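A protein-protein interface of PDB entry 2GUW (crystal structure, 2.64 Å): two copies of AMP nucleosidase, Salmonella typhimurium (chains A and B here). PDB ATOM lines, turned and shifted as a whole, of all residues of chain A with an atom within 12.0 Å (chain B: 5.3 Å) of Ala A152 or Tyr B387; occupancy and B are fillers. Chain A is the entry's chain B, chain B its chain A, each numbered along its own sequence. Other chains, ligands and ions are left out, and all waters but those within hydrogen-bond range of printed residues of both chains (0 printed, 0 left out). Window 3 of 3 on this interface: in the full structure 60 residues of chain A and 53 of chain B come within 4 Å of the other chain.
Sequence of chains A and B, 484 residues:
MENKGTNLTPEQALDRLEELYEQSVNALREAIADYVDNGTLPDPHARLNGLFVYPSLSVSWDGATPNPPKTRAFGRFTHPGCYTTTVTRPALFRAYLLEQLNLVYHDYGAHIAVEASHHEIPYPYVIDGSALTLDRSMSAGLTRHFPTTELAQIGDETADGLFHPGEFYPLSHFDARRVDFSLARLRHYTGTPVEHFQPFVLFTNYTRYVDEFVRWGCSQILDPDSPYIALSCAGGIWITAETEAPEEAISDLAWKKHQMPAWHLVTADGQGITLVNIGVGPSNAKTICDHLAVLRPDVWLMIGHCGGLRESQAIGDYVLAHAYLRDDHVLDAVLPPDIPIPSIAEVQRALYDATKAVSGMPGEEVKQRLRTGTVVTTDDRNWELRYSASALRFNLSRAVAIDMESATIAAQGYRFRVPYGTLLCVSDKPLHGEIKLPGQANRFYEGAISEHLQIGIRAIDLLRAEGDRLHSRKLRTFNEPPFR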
ATOM      1  N   HIS A 119      40.107   0.664   9.495  1.00  0.00           N
ATOM      2  CA  HIS A 119      39.723   0.669  10.902  1.00  0.00           C
ATOM      3  C   HIS A 119      40.718  -0.095  11.745  1.00  0.00           C
ATOM      4  O   HIS A 119      40.832  -1.312  11.612  1.00  0.00           O
ATOM      5  CB  HIS A 119      38.361   0.017  11.090  1.00  0.00           C
ATOM      6  CG  HIS A 119      37.280   0.625  10.260  1.00  0.00           C
ATOM      7  ND1 HIS A 119      37.003   1.973  10.273  1.00  0.00           N
ATOM      8  CD2 HIS A 119      36.401   0.065   9.394  1.00  0.00           C
ATOM      9  CE1 HIS A 119      36.002   2.218   9.447  1.00  0.00           C
ATOM     10  NE2 HIS A 119      35.618   1.078   8.901  1.00  0.00           N
ATOM     11  N   PRO A 122      41.102  -1.683  18.269  1.00  0.00           N
ATOM     12  CA  PRO A 122      41.349  -0.986  19.537  1.00  0.00           C
ATOM     13  C   PRO A 122      42.225  -1.865  20.438  1.00  0.00           C
ATOM     14  O   PRO A 122      41.876  -3.015  20.716  1.00  0.00           O
ATOM     15  CB  PRO A 122      39.946  -0.791  20.095  1.00  0.00           C
ATOM     16  CG  PRO A 122      39.121  -0.614  18.849  1.00  0.00           C
ATOM     17  CD  PRO A 122      39.664  -1.700  17.945  1.00  0.00           C
ATOM     18  N   TYR A 125      41.217  -4.768  22.610  1.00  0.00           N
ATOM     19  CA  TYR A 125      40.801  -6.011  21.977  1.00  0.00           C
ATOM     20  C   TYR A 125      41.934  -6.993  21.672  1.00  0.00           C
ATOM     21  O   TYR A 125      41.667  -8.112  21.245  1.00  0.00           O
ATOM     22  CB  TYR A 125      39.987  -5.733  20.706  1.00  0.00           C
ATOM     23  CG  TYR A 125      38.690  -4.983  20.953  1.00  0.00           C
ATOM     24  CD1 TYR A 125      37.888  -5.266  22.066  1.00  0.00           C
ATOM     25  CD2 TYR A 125      38.270  -3.975  20.082  1.00  0.00           C
ATOM     26  CE1 TYR A 125      36.700  -4.557  22.308  1.00  0.00           C
ATOM     27  CE2 TYR A 125      37.084  -3.262  20.310  1.00  0.00           C
ATOM     28  CZ  TYR A 125      36.309  -3.557  21.424  1.00  0.00           C
ATOM     29  OH  TYR A 125      35.154  -2.835  21.650  1.00  0.00           O
ATOM     30  N   THR A 148      41.798   3.324  19.958  1.00  0.00           N
ATOM     31  CA  THR A 148      40.865   3.103  21.053  1.00  0.00           C
ATOM     32  C   THR A 148      39.477   2.930  20.477  1.00  0.00           C
ATOM     33  O   THR A 148      39.288   3.004  19.270  1.00  0.00           O
ATOM     34  CB  THR A 148      40.819   4.301  22.006  1.00  0.00           C
ATOM     35  OG1 THR A 148      40.291   5.434  21.305  1.00  0.00           O
ATOM     36  CG2 THR A 148      42.208   4.631  22.533  1.00  0.00           C
ATOM     37  N   THR A 149      38.503   2.721  21.351  1.00  0.00           N
ATOM     38  CA  THR A 149      37.123   2.536  20.927  1.00  0.00           C
ATOM     39  C   THR A 149      36.407   3.875  20.789  1.00  0.00           C
ATOM     40  O   THR A 149      36.286   4.613  21.763  1.00  0.00           O
ATOM     41  CB  THR A 149      36.362   1.653  21.938  1.00  0.00           C
ATOM     42  OG1 THR A 149      36.354   2.287  23.225  1.00  0.00           O
ATOM     43  CG2 THR A 149      37.041   0.294  22.070  1.00  0.00           C
ATOM     44  N   GLU A 150      35.934   4.187  19.585  1.00  0.00           N
ATOM     45  CA  GLU A 150      35.229   5.450  19.349  1.00  0.00           C
ATOM     46  C   GLU A 150      33.806   5.254  18.828  1.00  0.00           C
ATOM     47  O   GLU A 150      33.592   5.101  17.621  1.00  0.00           O
ATOM     48  CB  GLU A 150      36.017   6.327  18.365  1.00  0.00           C
ATOM     49  CG  GLU A 150      37.313   6.923  18.941  1.00  0.00           C
ATOM     50  CD  GLU A 150      37.091   7.743  20.219  1.00  0.00           C
ATOM     51  OE1 GLU A 150      36.197   8.622  20.224  1.00  0.00           O
ATOM     52  OE2 GLU A 150      37.821   7.512  21.213  1.00  0.00           O
ATOM     53  N   LEU A 151      32.841   5.282  19.748  1.00  0.00           N
ATOM     54  CA  LEU A 151      31.420   5.091  19.442  1.00  0.00           C
ATOM     55  C   LEU A 151      30.903   5.973  18.308  1.00  0.00           C
ATOM     56  O   LEU A 151      30.406   5.475  17.293  1.00  0.00           O
ATOM     57  CB  LEU A 151      30.574   5.364  20.686  1.00  0.00           C
ATOM     58  CG  LEU A 151      31.149   4.939  22.035  1.00  0.00           C
ATOM     59  CD1 LEU A 151      32.324   5.840  22.408  1.00  0.00           C
ATOM     60  CD2 LEU A 151      30.066   5.038  23.088  1.00  0.00           C
ATOM     61  N   ALA A 152      31.006   7.286  18.505  1.00  0.00           N
ATOM     62  CA  ALA A 152      30.552   8.264  17.521  1.00  0.00           C
ATOM     63  C   ALA A 152      31.357   9.558  17.668  1.00  0.00           C
ATOM     64  O   ALA A 152      31.417  10.382  16.750  1.00  0.00           O
ATOM     65  CB  ALA A 152      29.055   8.543  17.714  1.00  0.00           C
ATOM     66  N   ASP A 175      29.736  -5.212  12.324  1.00  0.00           N
ATOM     67  CA  ASP A 175      31.107  -5.043  11.863  1.00  0.00           C
ATOM     68  C   ASP A 175      32.107  -5.450  12.946  1.00  0.00           C
ATOM     69  O   ASP A 175      31.735  -5.706  14.091  1.00  0.00           O
ATOM     70  CB  ASP A 175      31.349  -3.600  11.418  1.00  0.00           C
ATOM     71  CG  ASP A 175      31.406  -2.632  12.571  1.00  0.00           C
ATOM     72  OD1 ASP A 175      31.350  -1.409  12.315  1.00  0.00           O
ATOM     73  OD2 ASP A 175      31.520  -3.088  13.728  1.00  0.00           O
ATOM     74  N   ARG A 177      34.413  -4.000  14.981  1.00  0.00           N
ATOM     75  CA  ARG A 177      34.389  -3.358  16.302  1.00  0.00           C
ATOM     76  C   ARG A 177      33.124  -3.745  17.088  1.00  0.00           C
ATOM     77  O   ARG A 177      33.192  -4.009  18.300  1.00  0.00           O
ATOM     78  CB  ARG A 177      34.498  -1.830  16.162  1.00  0.00           C
ATOM     79  N   ARG A 178      31.981  -3.796  16.400  1.00  0.00           N
ATOM     80  CA  ARG A 178      30.729  -4.177  17.048  1.00  0.00           C
ATOM     81  C   ARG A 178      30.820  -5.601  17.569  1.00  0.00           C
ATOM     82  O   ARG A 178      30.333  -5.900  18.658  1.00  0.00           O
ATOM     83  CB  ARG A 178      29.558  -4.075  16.075  1.00  0.00           C
ATOM     84  CG  ARG A 178      28.287  -4.783  16.548  1.00  0.00           C
ATOM     85  CD  ARG A 178      27.772  -4.253  17.890  1.00  0.00           C
ATOM     86  NE  ARG A 178      27.214  -5.343  18.688  1.00  0.00           N
ATOM     87  CZ  ARG A 178      25.920  -5.560  18.871  1.00  0.00           C
ATOM     88  NH1 ARG A 178      25.013  -4.752  18.322  1.00  0.00           N
ATOM     89  NH2 ARG A 178      25.530  -6.604  19.584  1.00  0.00           N
ATOM     90  N   PHE A 181      33.454  -5.929  20.576  1.00  0.00           N
ATOM     91  CA  PHE A 181      32.769  -5.389  21.745  1.00  0.00           C
ATOM     92  C   PHE A 181      32.067  -6.544  22.495  1.00  0.00           C
ATOM     93  O   PHE A 181      32.373  -6.839  23.663  1.00  0.00           O
ATOM     94  CB  PHE A 181      31.743  -4.368  21.256  1.00  0.00           C
ATOM     95  CG  PHE A 181      30.821  -3.864  22.312  1.00  0.00           C
ATOM     96  CD1 PHE A 181      31.164  -2.765  23.087  1.00  0.00           C
ATOM     97  CD2 PHE A 181      29.593  -4.483  22.527  1.00  0.00           C
ATOM     98  CE1 PHE A 181      30.297  -2.277  24.069  1.00  0.00           C
ATOM     99  CE2 PHE A 181      28.718  -4.009  23.503  1.00  0.00           C
ATOM    100  CZ  PHE A 181      29.078  -2.899  24.277  1.00  0.00           C
ATOM    101  N   ARG A 185      33.021  -9.185  26.043  1.00  0.00           N
ATOM    102  CA  ARG A 185      32.145  -9.391  27.192  1.00  0.00           C
ATOM    103  C   ARG A 185      31.560 -10.790  27.411  1.00  0.00           C
ATOM    104  O   ARG A 185      31.390 -11.202  28.556  1.00  0.00           O
ATOM    105  CB  ARG A 185      31.025  -8.335  27.168  1.00  0.00           C
ATOM    106  CG  ARG A 185      31.599  -6.922  27.175  1.00  0.00           C
ATOM    107  CD  ARG A 185      30.579  -5.802  27.232  1.00  0.00           C
ATOM    108  NE  ARG A 185      31.239  -4.508  27.047  1.00  0.00           N
ATOM    109  CZ  ARG A 185      30.679  -3.322  27.292  1.00  0.00           C
ATOM    110  NH1 ARG A 185      29.431  -3.240  27.741  1.00  0.00           N
ATOM    111  NH2 ARG A 185      31.371  -2.208  27.087  1.00  0.00           N
ATOM    112  N   LYS A 286      18.360  -8.746  27.929  1.00  0.00           N
ATOM    113  CA  LYS A 286      18.703  -7.857  26.830  1.00  0.00           C
ATOM    114  C   LYS A 286      20.212  -7.891  26.593  1.00  0.00           C
ATOM    115  O   LYS A 286      20.674  -8.016  25.460  1.00  0.00           O
ATOM    116  CB  LYS A 286      18.261  -6.438  27.172  1.00  0.00           C
ATOM    117  CG  LYS A 286      18.189  -5.463  26.003  1.00  0.00           C
ATOM    118  CD  LYS A 286      19.529  -4.879  25.661  1.00  0.00           C
ATOM    119  CE  LYS A 286      19.356  -3.578  24.897  1.00  0.00           C
ATOM    120  NZ  LYS A 286      20.657  -2.873  24.695  1.00  0.00           N
ATOM    121  N   ASP A 290      22.443  -9.285  23.279  1.00  0.00           N
ATOM    122  CA  ASP A 290      23.190  -8.339  22.440  1.00  0.00           C
ATOM    123  C   ASP A 290      24.518  -8.963  22.008  1.00  0.00           C
ATOM    124  O   ASP A 290      24.954  -8.813  20.873  1.00  0.00           O
ATOM    125  CB  ASP A 290      23.521  -7.065  23.219  1.00  0.00           C
ATOM    126  CG  ASP A 290      22.404  -6.059  23.216  1.00  0.00           C
ATOM    127  OD1 ASP A 290      22.420  -5.193  24.121  1.00  0.00           O
ATOM    128  OD2 ASP A 290      21.538  -6.115  22.312  1.00  0.00           O
ATOM    129  N   ALA A 333      12.722   1.802  23.498  1.00  0.00           N
ATOM    130  CA  ALA A 333      13.319   2.779  22.609  1.00  0.00           C
ATOM    131  C   ALA A 333      13.690   2.230  21.234  1.00  0.00           C
ATOM    132  O   ALA A 333      13.403   2.868  20.219  1.00  0.00           O
ATOM    133  CB  ALA A 333      14.533   3.397  23.260  1.00  0.00           C
ATOM    134  N   VAL A 334      14.298   1.052  21.182  1.00  0.00           N
ATOM    135  CA  VAL A 334      14.714   0.517  19.893  1.00  0.00           C
ATOM    136  C   VAL A 334      13.684  -0.335  19.197  1.00  0.00           C
ATOM    137  O   VAL A 334      13.872  -0.720  18.046  1.00  0.00           O
ATOM    138  CB  VAL A 334      16.017  -0.302  20.012  1.00  0.00           C
ATOM    139  CG1 VAL A 334      17.140   0.591  20.464  1.00  0.00           C
ATOM    140  CG2 VAL A 334      15.816  -1.471  20.974  1.00  0.00           C
ATOM    141  N   ARG A 415      14.680  -8.965  16.765  1.00  0.00           N
ATOM    142  CA  ARG A 415      15.581  -7.923  16.260  1.00  0.00           C
ATOM    143  C   ARG A 415      16.804  -8.475  15.510  1.00  0.00           C
ATOM    144  O   ARG A 415      17.245  -7.888  14.516  1.00  0.00           O
ATOM    145  CB  ARG A 415      16.102  -7.020  17.392  1.00  0.00           C
ATOM    146  CG  ARG A 415      15.080  -6.131  18.060  1.00  0.00           C
ATOM    147  CD  ARG A 415      15.712  -4.784  18.435  1.00  0.00           C
ATOM    148  NE  ARG A 415      16.924  -4.968  19.220  1.00  0.00           N
ATOM    149  CZ  ARG A 415      17.937  -4.110  19.279  1.00  0.00           C
ATOM    150  NH1 ARG A 415      17.925  -2.967  18.598  1.00  0.00           N
ATOM    151  NH2 ARG A 415      18.980  -4.410  20.038  1.00  0.00           N
ATOM    152  N   TRP B 383      24.385   0.581  26.682  1.00  0.00           N
ATOM    153  CA  TRP B 383      23.962   1.879  26.171  1.00  0.00           C
ATOM    154  C   TRP B 383      24.913   2.388  25.081  1.00  0.00           C
ATOM    155  O   TRP B 383      24.500   3.125  24.178  1.00  0.00           O
ATOM    156  CB  TRP B 383      23.872   2.909  27.306  1.00  0.00           C
ATOM    157  CG  TRP B 383      25.137   3.073  28.009  1.00  0.00           C
ATOM    158  CD1 TRP B 383      25.650   2.255  28.967  1.00  0.00           C
ATOM    159  CD2 TRP B 383      26.092   4.103  27.796  1.00  0.00           C
ATOM    160  NE1 TRP B 383      26.876   2.717  29.376  1.00  0.00           N
ATOM    161  CE2 TRP B 383      27.176   3.852  28.672  1.00  0.00           C
ATOM    162  CE3 TRP B 383      26.143   5.220  26.950  1.00  0.00           C
ATOM    163  CZ2 TRP B 383      28.307   4.675  28.726  1.00  0.00           C
ATOM    164  CZ3 TRP B 383      27.266   6.042  27.000  1.00  0.00           C
ATOM    165  CH2 TRP B 383      28.334   5.762  27.882  1.00  0.00           C
ATOM    166  N   GLU B 384      26.183   1.996  25.168  1.00  0.00           N
ATOM    167  CA  GLU B 384      27.157   2.419  24.177  1.00  0.00           C
ATOM    168  C   GLU B 384      26.712   2.104  22.755  1.00  0.00           C
ATOM    169  O   GLU B 384      27.059   2.838  21.828  1.00  0.00           O
ATOM    170  CB  GLU B 384      28.512   1.770  24.441  1.00  0.00           C
ATOM    171  CG  GLU B 384      29.072   2.079  25.813  1.00  0.00           C
ATOM    172  CD  GLU B 384      28.891   0.934  26.791  1.00  0.00           C
ATOM    173  OE1 GLU B 384      27.745   0.430  26.930  1.00  0.00           O
ATOM    174  OE2 GLU B 384      29.909   0.550  27.417  1.00  0.00           O
ATOM    175  N   LEU B 385      25.951   1.025  22.565  1.00  0.00           N
ATOM    176  CA  LEU B 385      25.489   0.690  21.222  1.00  0.00           C
ATOM    177  C   LEU B 385      24.555   1.760  20.707  1.00  0.00           C
ATOM    178  O   LEU B 385      24.315   1.846  19.512  1.00  0.00           O
ATOM    179  CB  LEU B 385      24.753  -0.647  21.197  1.00  0.00           C
ATOM    180  CG  LEU B 385      25.543  -1.901  21.579  1.00  0.00           C
ATOM    181  CD1 LEU B 385      24.668  -3.151  21.377  1.00  0.00           C
ATOM    182  CD2 LEU B 385      26.817  -1.988  20.723  1.00  0.00           C
ATOM    183  N   ARG B 386      24.030   2.573  21.619  1.00  0.00           N
ATOM    184  CA  ARG B 386      23.093   3.650  21.279  1.00  0.00           C
ATOM    185  C   ARG B 386      23.563   5.029  21.729  1.00  0.00           C
ATOM    186  O   ARG B 386      22.734   5.890  22.027  1.00  0.00           O
ATOM    187  CB  ARG B 386      21.735   3.405  21.940  1.00  0.00           C
ATOM    188  CG  ARG B 386      20.820   2.453  21.235  1.00  0.00           C
ATOM    189  CD  ARG B 386      19.592   2.187  22.098  1.00  0.00           C
ATOM    190  NE  ARG B 386      18.784   3.378  22.338  1.00  0.00           N
ATOM    191  CZ  ARG B 386      18.212   4.098  21.376  1.00  0.00           C
ATOM    192  NH1 ARG B 386      18.362   3.749  20.095  1.00  0.00           N
ATOM    193  NH2 ARG B 386      17.478   5.162  21.696  1.00  0.00           N
ATOM    194  N   TYR B 387      24.868   5.254  21.794  1.00  0.00           N
ATOM    195  CA  TYR B 387      25.348   6.553  22.246  1.00  0.00           C
ATOM    196  C   TYR B 387      24.670   7.723  21.551  1.00  0.00           C
ATOM    197  O   TYR B 387      24.210   8.657  22.199  1.00  0.00           O
ATOM    198  CB  TYR B 387      26.866   6.684  22.063  1.00  0.00           C
ATOM    199  CG  TYR B 387      27.366   8.055  22.456  1.00  0.00           C
ATOM    200  CD1 TYR B 387      27.011   8.616  23.687  1.00  0.00           C
ATOM    201  CD2 TYR B 387      28.136   8.819  21.576  1.00  0.00           C
ATOM    202  CE1 TYR B 387      27.400   9.909  24.031  1.00  0.00           C
ATOM    203  CE2 TYR B 387      28.537  10.113  21.910  1.00  0.00           C
ATOM    204  CZ  TYR B 387      28.162  10.655  23.138  1.00  0.00           C
ATOM    205  OH  TYR B 387      28.525  11.946  23.458  1.00  0.00           O
ATOM    206  N   SER B 388      24.617   7.663  20.227  1.00  0.00           N
ATOM    207  CA  SER B 388      24.015   8.726  19.442  1.00  0.00           C
ATOM    208  C   SER B 388      22.698   9.214  20.016  1.00  0.00           C
ATOM    209  O   SER B 388      22.484  10.416  20.139  1.00  0.00           O
ATOM    210  CB  SER B 388      23.807   8.255  18.011  1.00  0.00           C
ATOM    211  OG  SER B 388      25.046   7.847  17.458  1.00  0.00           O
ATOM    212  N   ALA B 389      21.814   8.289  20.364  1.00  0.00           N
ATOM    213  CA  ALA B 389      20.529   8.662  20.936  1.00  0.00           C
ATOM    214  C   ALA B 389      20.705   9.265  22.339  1.00  0.00           C
ATOM    215  O   ALA B 389      20.223  10.360  22.620  1.00  0.00           O
ATOM    216  CB  ALA B 389      19.631   7.450  21.000  1.00  0.00           C
ATOM    217  N   SER B 390      21.417   8.557  23.206  1.00  0.00           N
ATOM    218  CA  SER B 390      21.645   9.009  24.569  1.00  0.00           C
ATOM    219  C   SER B 390      22.423  10.323  24.699  1.00  0.00           C
ATOM    220  O   SER B 390      22.313  11.025  25.707  1.00  0.00           O
ATOM    221  CB  SER B 390      22.384   7.920  25.341  1.00  0.00           C
ATOM    222  OG  SER B 390      21.646   6.711  25.334  1.00  0.00           O
ATOM    223  N   ALA B 391      23.207  10.654  23.680  1.00  0.00           N
ATOM    224  CA  ALA B 391      24.030  11.865  23.687  1.00  0.00           C
ATOM    225  C   ALA B 391      23.326  13.140  24.184  1.00  0.00           C
ATOM    226  O   ALA B 391      23.792  13.795  25.128  1.00  0.00           O
ATOM    227  CB  ALA B 391      24.619  12.091  22.282  1.00  0.00           C
ATOM    228  N   PHE B 394      22.329  13.085  27.866  1.00  0.00           N
ATOM    229  CA  PHE B 394      23.498  13.124  28.739  1.00  0.00           C
ATOM    230  C   PHE B 394      23.978  14.565  28.814  1.00  0.00           C
ATOM    231  O   PHE B 394      24.370  15.035  29.886  1.00  0.00           O
ATOM    232  CB  PHE B 394      24.618  12.234  28.198  1.00  0.00           C
ATOM    233  CG  PHE B 394      24.405  10.759  28.419  1.00  0.00           C
ATOM    234  CD1 PHE B 394      23.137  10.242  28.703  1.00  0.00           C
ATOM    235  CD2 PHE B 394      25.476   9.880  28.309  1.00  0.00           C
ATOM    236  CE1 PHE B 394      22.940   8.872  28.876  1.00  0.00           C
ATOM    237  CE2 PHE B 394      25.298   8.509  28.478  1.00  0.00           C
ATOM    238  CZ  PHE B 394      24.026   8.000  28.765  1.00  0.00           C
ATOM    239  N   ASN B 395      23.930  15.261  27.674  1.00  0.00           N
ATOM    240  CA  ASN B 395      24.352  16.656  27.599  1.00  0.00           C
ATOM    241  C   ASN B 395      23.415  17.600  28.355  1.00  0.00           C
ATOM    242  O   ASN B 395      23.875  18.489  29.082  1.00  0.00           O
ATOM    243  CB  ASN B 395      24.471  17.102  26.147  1.00  0.00           C
ATOM    244  CG  ASN B 395      25.571  16.352  25.388  1.00  0.00           C
ATOM    245  OD1 ASN B 395      26.525  15.833  25.984  1.00  0.00           O
ATOM    246  ND2 ASN B 395      25.449  16.310  24.061  1.00  0.00           N
ATOM    247  N   LEU B 431      33.265   7.096  26.581  1.00  0.00           N
ATOM    248  CA  LEU B 431      33.350   8.081  25.510  1.00  0.00           C
ATOM    249  C   LEU B 431      34.739   8.662  25.290  1.00  0.00           C
ATOM    250  O   LEU B 431      34.886   9.656  24.583  1.00  0.00           O
ATOM    251  CB  LEU B 431      32.377   9.242  25.760  1.00  0.00           C
ATOM    252  CG  LEU B 431      30.855   9.039  25.773  1.00  0.00           C
ATOM    253  CD1 LEU B 431      30.478   7.747  25.073  1.00  0.00           C
ATOM    254  CD2 LEU B 431      30.367   9.027  27.204  1.00  0.00           C
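Of chain B, only Tyr B387 comes within 4 Å of Ala A152. Printed residues of chain A within 4 Å of Tyr B387: Leu A151 and Ala A152. Of chain A, only Ala A333 (3.8 Å) and Val A334 (3.4 Å) come within 4 Å of Arg B386. No residue of chain A comes within 4 Å of Ala B391. Leu B431 touches just one residue of chain A: Leu A151 (3.4 Å). Printed residues of chain A within 4 Å of Glu B384: Leu A151 (3.9 Å) and Arg A185 (3.1 Å). Printed residues of chain B within 4 Å of Arg A178: Leu B385 (3.5 Å). Of the printed residues of chain B, Arg A185 touches Glu B384 (3.1 Å). Printed residues of chain A within 4 Å of Leu B385: Arg A178 and Phe A181. Arg A415 touches none of the printed residues of chain B. The nearest residue of chain A that does not touch Tyr B387 is Glu A150 (7.2 Å). The nearest printed residue of chain B that does not touch Arg A178 is Glu B384 (8.1 Å).
The indole nitrogen (NE1) of Trp B383 lies close to the side-chain carboxylate (OE1) of Glu B384 (3.5 Å). The side-chain carboxylate (OD2) of Asp A175 is in hydrogen-bond range of the backbone NH (N) of Arg A178, 2.8 Å away. The backbone carbonyl oxygen (O) of Asp A290 lies within hydrogen-bond range of the guanidinium group (NH2) of Arg A178, 2.6 Å away.
Hydrophobic or aromatic side chains of chain A within 4 Å of the printed part of chain B: Leu A151, Ala A152, Phe A181, Ala A333 and Val A334. Among the printed residues, 9 pairs touch across the chains.
No position is printed for both chains. Of the 9 pairs that touch across the chains among the printed residues, none has its exchanged pair printed and touching as well.
OE2 of Glu B384 is in salt-bridge range of NH2 of Arg A185.
Among the printed residues, merely in contact across the chains: Val A334 with Arg B386, Leu A151 with Leu B431, Arg A178 with Leu B385, Leu A151 with Tyr B387, Ala A333 with Arg B386, Leu A151 with Glu B384, Phe A181 with Leu B385 and Ala A152 with Tyr B387.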
